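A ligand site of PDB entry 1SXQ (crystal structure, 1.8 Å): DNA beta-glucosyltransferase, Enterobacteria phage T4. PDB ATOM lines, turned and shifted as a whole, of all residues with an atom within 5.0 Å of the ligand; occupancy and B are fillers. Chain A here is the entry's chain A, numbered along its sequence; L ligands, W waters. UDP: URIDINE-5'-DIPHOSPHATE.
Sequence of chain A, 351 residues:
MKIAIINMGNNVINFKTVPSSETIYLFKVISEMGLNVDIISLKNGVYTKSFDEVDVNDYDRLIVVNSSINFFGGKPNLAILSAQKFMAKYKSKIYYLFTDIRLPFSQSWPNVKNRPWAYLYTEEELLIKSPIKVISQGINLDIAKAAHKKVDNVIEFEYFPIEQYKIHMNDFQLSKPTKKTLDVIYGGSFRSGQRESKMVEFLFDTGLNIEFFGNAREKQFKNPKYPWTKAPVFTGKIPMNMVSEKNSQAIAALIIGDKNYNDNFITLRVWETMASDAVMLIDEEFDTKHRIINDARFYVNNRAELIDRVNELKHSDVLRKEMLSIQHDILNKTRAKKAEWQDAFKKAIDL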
ATOM      1  N   VAL A  18     -11.914 -33.403 -19.690  1.00  0.00           N
ATOM      2  CA  VAL A  18     -11.067 -33.151 -20.846  1.00  0.00           C
ATOM      3  C   VAL A  18      -9.995 -34.226 -21.075  1.00  0.00           C
ATOM      4  O   VAL A  18      -9.800 -34.692 -22.199  1.00  0.00           O
ATOM      5  CB  VAL A  18     -10.415 -31.755 -20.764  1.00  0.00           C
ATOM      6  CG1 VAL A  18      -9.508 -31.520 -21.975  1.00  0.00           C
ATOM      7  CG2 VAL A  18     -11.495 -30.689 -20.701  1.00  0.00           C
ATOM      8  N   ASP A 100       0.641 -30.464 -24.433  1.00  0.00           N
ATOM      9  CA  ASP A 100       0.577 -29.317 -23.530  1.00  0.00           C
ATOM     10  C   ASP A 100       1.979 -29.098 -22.973  1.00  0.00           C
ATOM     11  O   ASP A 100       2.538 -29.971 -22.320  1.00  0.00           O
ATOM     12  CB  ASP A 100      -0.417 -29.599 -22.396  1.00  0.00           C
ATOM     13  CG  ASP A 100      -0.639 -28.400 -21.479  1.00  0.00           C
ATOM     14  OD1 ASP A 100      -1.765 -28.280 -20.941  1.00  0.00           O
ATOM     15  OD2 ASP A 100       0.296 -27.597 -21.283  1.00  0.00           O
ATOM     16  N   ARG A 102       3.062 -27.646 -20.501  1.00  0.00           N
ATOM     17  CA  ARG A 102       3.188 -27.782 -19.044  1.00  0.00           C
ATOM     18  C   ARG A 102       3.303 -29.241 -18.580  1.00  0.00           C
ATOM     19  O   ARG A 102       3.604 -29.497 -17.414  1.00  0.00           O
ATOM     20  CB  ARG A 102       1.958 -27.192 -18.338  1.00  0.00           C
ATOM     21  CG  ARG A 102       1.562 -25.765 -18.682  1.00  0.00           C
ATOM     22  CD  ARG A 102       0.197 -25.486 -18.038  1.00  0.00           C
ATOM     23  NE  ARG A 102      -0.796 -26.469 -18.477  1.00  0.00           N
ATOM     24  CZ  ARG A 102      -1.939 -26.729 -17.844  1.00  0.00           C
ATOM     25  NH1 ARG A 102      -2.767 -27.645 -18.341  1.00  0.00           N
ATOM     26  NH2 ARG A 102      -2.267 -26.098 -16.724  1.00  0.00           N
ATOM     27  N   TYR A 186     -14.670 -17.516 -24.987  1.00  0.00           N
ATOM     28  CA  TYR A 186     -13.421 -18.228 -24.832  1.00  0.00           C
ATOM     29  C   TYR A 186     -13.637 -19.318 -23.801  1.00  0.00           C
ATOM     30  O   TYR A 186     -14.155 -19.062 -22.715  1.00  0.00           O
ATOM     31  CB  TYR A 186     -12.301 -17.277 -24.359  1.00  0.00           C
ATOM     32  CG  TYR A 186     -10.986 -17.962 -24.044  1.00  0.00           C
ATOM     33  CD1 TYR A 186     -10.741 -18.499 -22.786  1.00  0.00           C
ATOM     34  CD2 TYR A 186      -9.989 -18.072 -25.013  1.00  0.00           C
ATOM     35  CE1 TYR A 186      -9.514 -19.120 -22.492  1.00  0.00           C
ATOM     36  CE2 TYR A 186      -8.762 -18.691 -24.734  1.00  0.00           C
ATOM     37  CZ  TYR A 186      -8.539 -19.209 -23.472  1.00  0.00           C
ATOM     38  OH  TYR A 186      -7.341 -19.818 -23.190  1.00  0.00           O
ATOM     39  N   GLY A 187     -13.258 -20.546 -24.133  1.00  0.00           N
ATOM     40  CA  GLY A 187     -13.427 -21.648 -23.206  1.00  0.00           C
ATOM     41  C   GLY A 187     -12.098 -22.273 -22.831  1.00  0.00           C
ATOM     42  O   GLY A 187     -11.292 -22.619 -23.690  1.00  0.00           O
ATOM     43  N   GLY A 188     -11.847 -22.415 -21.529  1.00  0.00           N
ATOM     44  CA  GLY A 188     -10.595 -23.010 -21.103  1.00  0.00           C
ATOM     45  C   GLY A 188     -10.424 -22.939 -19.612  1.00  0.00           C
ATOM     46  O   GLY A 188     -11.329 -22.505 -18.893  1.00  0.00           O
ATOM     47  N   SER A 189      -9.269 -23.381 -19.136  1.00  0.00           N
ATOM     48  CA  SER A 189      -8.978 -23.364 -17.709  1.00  0.00           C
ATOM     49  C   SER A 189      -8.054 -22.180 -17.449  1.00  0.00           C
ATOM     50  O   SER A 189      -7.624 -21.493 -18.375  1.00  0.00           O
ATOM     51  CB  SER A 189      -8.296 -24.651 -17.271  1.00  0.00           C
ATOM     52  OG  SER A 189      -6.980 -24.722 -17.793  1.00  0.00           O
ATOM     53  N   ARG A 191      -5.106 -22.477 -16.356  1.00  0.00           N
ATOM     54  CA  ARG A 191      -3.749 -22.910 -16.689  1.00  0.00           C
ATOM     55  C   ARG A 191      -2.722 -22.374 -15.687  1.00  0.00           C
ATOM     56  O   ARG A 191      -1.612 -22.006 -16.057  1.00  0.00           O
ATOM     57  CB  ARG A 191      -3.383 -22.469 -18.112  1.00  0.00           C
ATOM     58  CG  ARG A 191      -4.211 -23.173 -19.191  1.00  0.00           C
ATOM     59  CD  ARG A 191      -3.733 -22.814 -20.596  1.00  0.00           C
ATOM     60  NE  ARG A 191      -2.327 -23.188 -20.806  1.00  0.00           N
ATOM     61  CZ  ARG A 191      -1.907 -24.434 -20.977  1.00  0.00           C
ATOM     62  NH1 ARG A 191      -2.766 -25.444 -20.987  1.00  0.00           N
ATOM     63  NH2 ARG A 191      -0.609 -24.673 -21.125  1.00  0.00           N
ATOM     64  N   ARG A 195      -1.287 -17.784 -18.679  1.00  0.00           N
ATOM     65  CA  ARG A 195      -1.787 -16.954 -19.758  1.00  0.00           C
ATOM     66  C   ARG A 195      -2.619 -15.783 -19.219  1.00  0.00           C
ATOM     67  O   ARG A 195      -3.415 -15.188 -19.940  1.00  0.00           O
ATOM     68  CB  ARG A 195      -2.656 -17.847 -20.659  1.00  0.00           C
ATOM     69  CG  ARG A 195      -2.966 -17.344 -22.035  1.00  0.00           C
ATOM     70  CD  ARG A 195      -3.754 -18.431 -22.778  1.00  0.00           C
ATOM     71  NE  ARG A 195      -2.974 -19.661 -22.959  1.00  0.00           N
ATOM     72  CZ  ARG A 195      -3.438 -20.765 -23.543  1.00  0.00           C
ATOM     73  NH1 ARG A 195      -4.684 -20.813 -24.004  1.00  0.00           N
ATOM     74  NH2 ARG A 195      -2.639 -21.817 -23.709  1.00  0.00           N
ATOM     75  N   PHE A 213     -16.048 -19.663 -20.572  1.00  0.00           N
ATOM     76  CA  PHE A 213     -16.513 -20.935 -20.036  1.00  0.00           C
ATOM     77  C   PHE A 213     -15.362 -21.883 -19.759  1.00  0.00           C
ATOM     78  O   PHE A 213     -14.262 -21.720 -20.292  1.00  0.00           O
ATOM     79  CB  PHE A 213     -17.557 -21.599 -20.958  1.00  0.00           C
ATOM     80  CG  PHE A 213     -17.031 -22.077 -22.289  1.00  0.00           C
ATOM     81  CD1 PHE A 213     -16.860 -21.194 -23.353  1.00  0.00           C
ATOM     82  CD2 PHE A 213     -16.753 -23.423 -22.487  1.00  0.00           C
ATOM     83  CE1 PHE A 213     -16.434 -21.653 -24.605  1.00  0.00           C
ATOM     84  CE2 PHE A 213     -16.327 -23.895 -23.734  1.00  0.00           C
ATOM     85  CZ  PHE A 213     -16.173 -23.011 -24.797  1.00  0.00           C
ATOM     86  N   GLY A 214     -15.602 -22.875 -18.912  1.00  0.00           N
ATOM     87  CA  GLY A 214     -14.558 -23.824 -18.553  1.00  0.00           C
ATOM     88  C   GLY A 214     -14.205 -23.786 -17.081  1.00  0.00           C
ATOM     89  O   GLY A 214     -14.941 -23.243 -16.270  1.00  0.00           O
ATOM     90  N   GLY A 236     -19.711 -22.463 -16.103  1.00  0.00           N
ATOM     91  CA  GLY A 236     -19.042 -23.724 -15.862  1.00  0.00           C
ATOM     92  C   GLY A 236     -18.414 -24.410 -17.066  1.00  0.00           C
ATOM     93  O   GLY A 236     -18.520 -23.955 -18.198  1.00  0.00           O
ATOM     94  N   LYS A 237     -17.739 -25.524 -16.793  1.00  0.00           N
ATOM     95  CA  LYS A 237     -17.111 -26.281 -17.865  1.00  0.00           C
ATOM     96  C   LYS A 237     -18.170 -27.135 -18.553  1.00  0.00           C
ATOM     97  O   LYS A 237     -19.201 -27.444 -17.953  1.00  0.00           O
ATOM     98  CB  LYS A 237     -16.014 -27.199 -17.294  1.00  0.00           C
ATOM     99  CG  LYS A 237     -16.514 -28.252 -16.327  1.00  0.00           C
ATOM    100  CD  LYS A 237     -15.357 -29.095 -15.810  1.00  0.00           C
ATOM    101  CE  LYS A 237     -15.828 -30.102 -14.779  1.00  0.00           C
ATOM    102  NZ  LYS A 237     -14.690 -30.903 -14.254  1.00  0.00           N
ATOM    103  N   ILE A 238     -17.915 -27.491 -19.797  1.00  0.00           N
ATOM    104  CA  ILE A 238     -18.842 -28.314 -20.563  1.00  0.00           C
ATOM    105  C   ILE A 238     -18.040 -29.435 -21.192  1.00  0.00           C
ATOM    106  O   ILE A 238     -16.810 -29.367 -21.258  1.00  0.00           O
ATOM    107  CB  ILE A 238     -19.542 -27.511 -21.661  1.00  0.00           C
ATOM    108  CG1 ILE A 238     -18.517 -27.032 -22.691  1.00  0.00           C
ATOM    109  CG2 ILE A 238     -20.270 -26.315 -21.065  1.00  0.00           C
ATOM    110  CD1 ILE A 238     -19.141 -26.456 -23.937  1.00  0.00           C
ATOM    111  N   PRO A 239     -18.721 -30.492 -21.661  1.00  0.00           N
ATOM    112  CA  PRO A 239     -18.023 -31.617 -22.295  1.00  0.00           C
ATOM    113  C   PRO A 239     -17.259 -31.168 -23.522  1.00  0.00           C
ATOM    114  O   PRO A 239     -17.698 -30.268 -24.247  1.00  0.00           O
ATOM    115  CB  PRO A 239     -19.162 -32.582 -22.647  1.00  0.00           C
ATOM    116  CG  PRO A 239     -20.212 -32.279 -21.615  1.00  0.00           C
ATOM    117  CD  PRO A 239     -20.166 -30.766 -21.551  1.00  0.00           C
ATOM    118  N   MET A 240     -16.109 -31.796 -23.758  1.00  0.00           N
ATOM    119  CA  MET A 240     -15.296 -31.437 -24.916  1.00  0.00           C
ATOM    120  C   MET A 240     -16.066 -31.583 -26.213  1.00  0.00           C
ATOM    121  O   MET A 240     -15.862 -30.809 -27.160  1.00  0.00           O
ATOM    122  CB  MET A 240     -14.050 -32.315 -24.961  1.00  0.00           C
ATOM    123  CG  MET A 240     -13.067 -31.901 -26.029  1.00  0.00           C
ATOM    124  SD  MET A 240     -11.537 -32.850 -25.958  1.00  0.00           S
ATOM    125  CE  MET A 240     -10.964 -32.632 -27.584  1.00  0.00           C
ATOM    126  N   VAL A 243     -18.068 -28.349 -27.250  1.00  0.00           N
ATOM    127  CA  VAL A 243     -17.345 -27.080 -27.336  1.00  0.00           C
ATOM    128  C   VAL A 243     -17.624 -26.219 -28.560  1.00  0.00           C
ATOM    129  O   VAL A 243     -17.817 -25.012 -28.439  1.00  0.00           O
ATOM    130  CB  VAL A 243     -15.821 -27.311 -27.210  1.00  0.00           C
ATOM    131  CG1 VAL A 243     -15.072 -26.018 -27.529  1.00  0.00           C
ATOM    132  CG2 VAL A 243     -15.482 -27.764 -25.798  1.00  0.00           C
ATOM    133  N   ILE A 256      -5.755 -17.403 -28.149  1.00  0.00           N
ATOM    134  CA  ILE A 256      -4.560 -16.925 -27.456  1.00  0.00           C
ATOM    135  C   ILE A 256      -3.857 -18.182 -26.979  1.00  0.00           C
ATOM    136  O   ILE A 256      -4.426 -19.266 -26.983  1.00  0.00           O
ATOM    137  CB  ILE A 256      -4.876 -16.030 -26.235  1.00  0.00           C
ATOM    138  CG1 ILE A 256      -5.978 -16.669 -25.380  1.00  0.00           C
ATOM    139  CG2 ILE A 256      -5.273 -14.624 -26.698  1.00  0.00           C
ATOM    140  CD1 ILE A 256      -6.183 -16.001 -24.042  1.00  0.00           C
ATOM    141  N   TYR A 261       3.782 -21.110 -26.976  1.00  0.00           N
ATOM    142  CA  TYR A 261       2.933 -21.615 -28.050  1.00  0.00           C
ATOM    143  C   TYR A 261       3.040 -20.710 -29.265  1.00  0.00           C
ATOM    144  O   TYR A 261       2.750 -21.137 -30.395  1.00  0.00           O
ATOM    145  CB  TYR A 261       1.471 -21.673 -27.609  1.00  0.00           C
ATOM    146  CG  TYR A 261       1.132 -22.805 -26.667  1.00  0.00           C
ATOM    147  CD1 TYR A 261       2.079 -23.797 -26.355  1.00  0.00           C
ATOM    148  CD2 TYR A 261      -0.143 -22.929 -26.114  1.00  0.00           C
ATOM    149  CE1 TYR A 261       1.757 -24.861 -25.531  1.00  0.00           C
ATOM    150  CE2 TYR A 261      -0.477 -23.997 -25.284  1.00  0.00           C
ATOM    151  CZ  TYR A 261       0.482 -24.956 -25.002  1.00  0.00           C
ATOM    152  OH  TYR A 261       0.155 -26.015 -24.185  1.00  0.00           O
ATOM    153  N   THR A 267      -3.214 -25.163 -31.476  1.00  0.00           N
ATOM    154  CA  THR A 267      -3.975 -25.851 -30.439  1.00  0.00           C
ATOM    155  C   THR A 267      -5.353 -26.301 -30.884  1.00  0.00           C
ATOM    156  O   THR A 267      -5.867 -25.860 -31.912  1.00  0.00           O
ATOM    157  CB  THR A 267      -4.115 -24.933 -29.213  1.00  0.00           C
ATOM    158  OG1 THR A 267      -4.625 -23.674 -29.639  1.00  0.00           O
ATOM    159  CG2 THR A 267      -2.760 -24.718 -28.534  1.00  0.00           C
ATOM    160  N   LEU A 268      -5.947 -27.186 -30.086  1.00  0.00           N
ATOM    161  CA  LEU A 268      -7.279 -27.708 -30.394  1.00  0.00           C
ATOM    162  C   LEU A 268      -8.280 -26.578 -30.610  1.00  0.00           C
ATOM    163  O   LEU A 268      -9.097 -26.646 -31.527  1.00  0.00           O
ATOM    164  CB  LEU A 268      -7.760 -28.605 -29.251  1.00  0.00           C
ATOM    165  CG  LEU A 268      -8.603 -29.850 -29.559  1.00  0.00           C
ATOM    166  CD1 LEU A 268      -9.696 -29.520 -30.543  1.00  0.00           C
ATOM    167  CD2 LEU A 268      -7.720 -30.942 -30.122  1.00  0.00           C
ATOM    168  N   ARG A 269      -8.216 -25.543 -29.766  1.00  0.00           N
ATOM    169  CA  ARG A 269      -9.169 -24.441 -29.888  1.00  0.00           C
ATOM    170  C   ARG A 269      -9.127 -23.788 -31.258  1.00  0.00           C
ATOM    171  O   ARG A 269     -10.135 -23.248 -31.715  1.00  0.00           O
ATOM    172  CB  ARG A 269      -8.952 -23.385 -28.787  1.00  0.00           C
ATOM    173  CG  ARG A 269      -7.738 -22.503 -28.946  1.00  0.00           C
ATOM    174  CD  ARG A 269      -7.750 -21.364 -27.917  1.00  0.00           C
ATOM    175  NE  ARG A 269      -7.717 -21.845 -26.542  1.00  0.00           N
ATOM    176  CZ  ARG A 269      -8.780 -21.982 -25.755  1.00  0.00           C
ATOM    177  NH1 ARG A 269      -9.994 -21.667 -26.192  1.00  0.00           N
ATOM    178  NH2 ARG A 269      -8.629 -22.438 -24.516  1.00  0.00           N
ATOM    179  N   GLU A 272     -11.441 -26.032 -33.075  1.00  0.00           N
ATOM    180  CA  GLU A 272     -12.776 -25.955 -32.479  1.00  0.00           C
ATOM    181  C   GLU A 272     -13.437 -24.612 -32.786  1.00  0.00           C
ATOM    182  O   GLU A 272     -14.658 -24.520 -32.895  1.00  0.00           O
ATOM    183  CB  GLU A 272     -12.708 -26.118 -30.960  1.00  0.00           C
ATOM    184  CG  GLU A 272     -12.143 -27.441 -30.496  1.00  0.00           C
ATOM    185  CD  GLU A 272     -11.932 -27.472 -28.988  1.00  0.00           C
ATOM    186  OE1 GLU A 272     -11.617 -26.414 -28.406  1.00  0.00           O
ATOM    187  OE2 GLU A 272     -12.075 -28.563 -28.390  1.00  0.00           O
HETATM  188  N1  UDP L   1     -12.554 -27.438 -22.922  1.00  0.00           N
HETATM  189  C2  UDP L   1     -13.629 -28.274 -22.703  1.00  0.00           C
HETATM  190  N3  UDP L   1     -14.641 -27.741 -21.956  1.00  0.00           N
HETATM  191  C4  UDP L   1     -14.694 -26.460 -21.418  1.00  0.00           C
HETATM  192  C5  UDP L   1     -13.549 -25.647 -21.709  1.00  0.00           C
HETATM  193  C6  UDP L   1     -12.540 -26.155 -22.429  1.00  0.00           C
HETATM  194  O2  UDP L   1     -13.682 -29.414 -23.142  1.00  0.00           O
HETATM  195  O4  UDP L   1     -15.641 -26.149 -20.689  1.00  0.00           O
HETATM  196  C1' UDP L   1     -11.428 -27.983 -23.703  1.00  0.00           C
HETATM  197  C2' UDP L   1     -11.500 -27.637 -25.199  1.00  0.00           C
HETATM  198  O2' UDP L   1     -11.127 -28.761 -25.958  1.00  0.00           O
HETATM  199  C3' UDP L   1     -10.492 -26.498 -25.309  1.00  0.00           C
HETATM  200  C4' UDP L   1      -9.437 -26.892 -24.298  1.00  0.00           C
HETATM  201  O4' UDP L   1     -10.204 -27.451 -23.203  1.00  0.00           O
HETATM  202  O3' UDP L   1      -9.907 -26.417 -26.592  1.00  0.00           O
HETATM  203  C5' UDP L   1      -8.581 -25.747 -23.813  1.00  0.00           C
HETATM  204  O5' UDP L   1      -7.658 -26.185 -22.820  1.00  0.00           O
HETATM  205  PA  UDP L   1      -6.716 -25.136 -22.074  1.00  0.00           P
HETATM  206  O1A UDP L   1      -7.580 -24.343 -21.160  1.00  0.00           O
HETATM  207  O2A UDP L   1      -5.537 -25.857 -21.530  1.00  0.00           O
HETATM  208  O3A UDP L   1      -6.252 -24.127 -23.263  1.00  0.00           O
HETATM  209  PB  UDP L   1      -5.212 -24.352 -24.511  1.00  0.00           P
HETATM  210  O1B UDP L   1      -5.606 -25.662 -25.168  1.00  0.00           O
HETATM  211  O2B UDP L   1      -3.825 -24.378 -23.902  1.00  0.00           O
HETATM  212  O3B UDP L   1      -5.451 -23.149 -25.407  1.00  0.00           O
HETATM  213  O   HOH W   1      -5.589 -28.344 -25.213  1.00  0.00           O
HETATM  214  O   HOH W   2      -4.471 -28.294 -22.861  1.00  0.00           O
HETATM  215  O   HOH W   3      -7.168 -21.562 -21.112  1.00  0.00           O
HETATM  216  O   HOH W   4      -6.078 -26.960 -19.200  1.00  0.00           O
HETATM  217  O   HOH W   5      -4.230 -22.058 -27.511  1.00  0.00           O
HETATM  218  O   HOH W   6      -2.389 -26.542 -24.138  1.00  0.00           O
HETATM  219  O   HOH W   7      -9.676 -26.660 -20.457  1.00  0.00           O
HETATM  220  O   HOH W   8      -7.134 -25.726 -27.215  1.00  0.00           O
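Val 18 touches the ligand. C of Gly 187 touches C5 of the ligand, at 3.8 Å. CA of Gly 188 touches O1A of the ligand, 3.3 Å away. Phe 213 touches the ligand (CD2 to O4, 3.4 Å). Gly 214 touches the ligand. Lys 237 touches the ligand (CA to O4, 3.2 Å). Val 243 touches the ligand. Tyr 261 touches the ligand. Hydrophobic or aromatic side chains that line the ligand: Val 18, Phe 213, Ile 238, Met 240, Val 243 and Tyr 261. The nearest printed residue that does not touch the ligand is Pro 239 (4.002 Å).
The backbone carbonyl oxygen (O) of Ile 256 lies within hydrogen-bond range of the guanidinium group (NH1) of Arg 195 (3.4 Å). The guanidinium group (NH1) of Arg 195 is in hydrogen-bond range of the side-chain hydroxyl (OH) of Tyr 186, at 3.0 Å. NH2 of Arg 269 lies within hydrogen-bond range of O of Gly 187, 2.8 Å away. NH2 of Arg 269 sits at hydrogen-bond distance from OH of Tyr 186 (3.2 Å). N of Gly 188 lies within hydrogen-bond range of O of Phe 213 (2.8 Å). The backbone NH (N) of Gly 214 lies within hydrogen-bond range of the backbone carbonyl oxygen (O) of Gly 236 (3.2 Å). N of Phe 213 sits at hydrogen-bond distance from O of Tyr 186, 2.9 Å away. The side-chain carboxylate of Asp 100 sits at hydrogen-bond distance from the side-chain hydroxyl of Tyr 261, at 3.3 Å.
The side-chain carboxylate (OE1) of Glu 272 is in hydrogen-bond range of an oxygen (O3') of the ligand (2.5 Å). The backbone NH (N) of Ile 238 lies within hydrogen-bond range of an oxygen (O4) of the ligand (2.8 Å). N3 of the ligand is in hydrogen-bond range of O of Ile 238, 2.8 Å away. An oxygen (O1A) of the ligand lies within hydrogen-bond range of the backbone NH (N) of Ser 189 (2.8 Å). OG of Ser 189 sits at hydrogen-bond distance from O1A of the ligand (3.4 Å). NH2 of Arg 195 lies within salt-bridge range of O2B of the ligand (2.8 Å). The guanidinium group (NE) of Arg 269 lies within salt-bridge range of an oxygen (O3B) of the ligand (2.9 Å). An oxygen (O2A) of the ligand is in salt-bridge range of the guanidinium group (NH1) of Arg 191 (2.9 Å). The backbone NH (N) of Met 240 lies close to an oxygen (O2) of the ligand (3.5 Å).
Water W8 lies within hydrogen-bond range of O1B of the ligand (2.6 Å), N of Arg 269 (2.8 Å) and N of Leu 268 (3.4 Å). Water W6 lies within hydrogen-bond range of the side-chain hydroxyl of Tyr 261, an oxygen (O2B) of the ligand and the guanidinium group of Arg 191. Water W4 lies within hydrogen-bond range of an oxygen (O2A) of the ligand (2.6 Å), the side-chain hydroxyl of Ser 189 (2.8 Å) and the guanidinium group of Arg 102 (3.5 Å). Water W5 lies within hydrogen-bond range of an oxygen (O3B) of the ligand (2.7 Å), the side-chain hydroxyl of Thr 267 (2.7 Å) and the backbone carbonyl oxygen of Ile 256 (2.8 Å). Water W3 lies within hydrogen-bond range of the side-chain hydroxyl (OH) of Tyr 186 (2.7 Å), the backbone carbonyl oxygen (O) of Ser 189 (2.8 Å) and an oxygen (O1A) of the ligand (2.8 Å). Water W2 bridges O2A of the ligand (3.0 Å) and OD1 of Asp 100 (3.3 Å).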
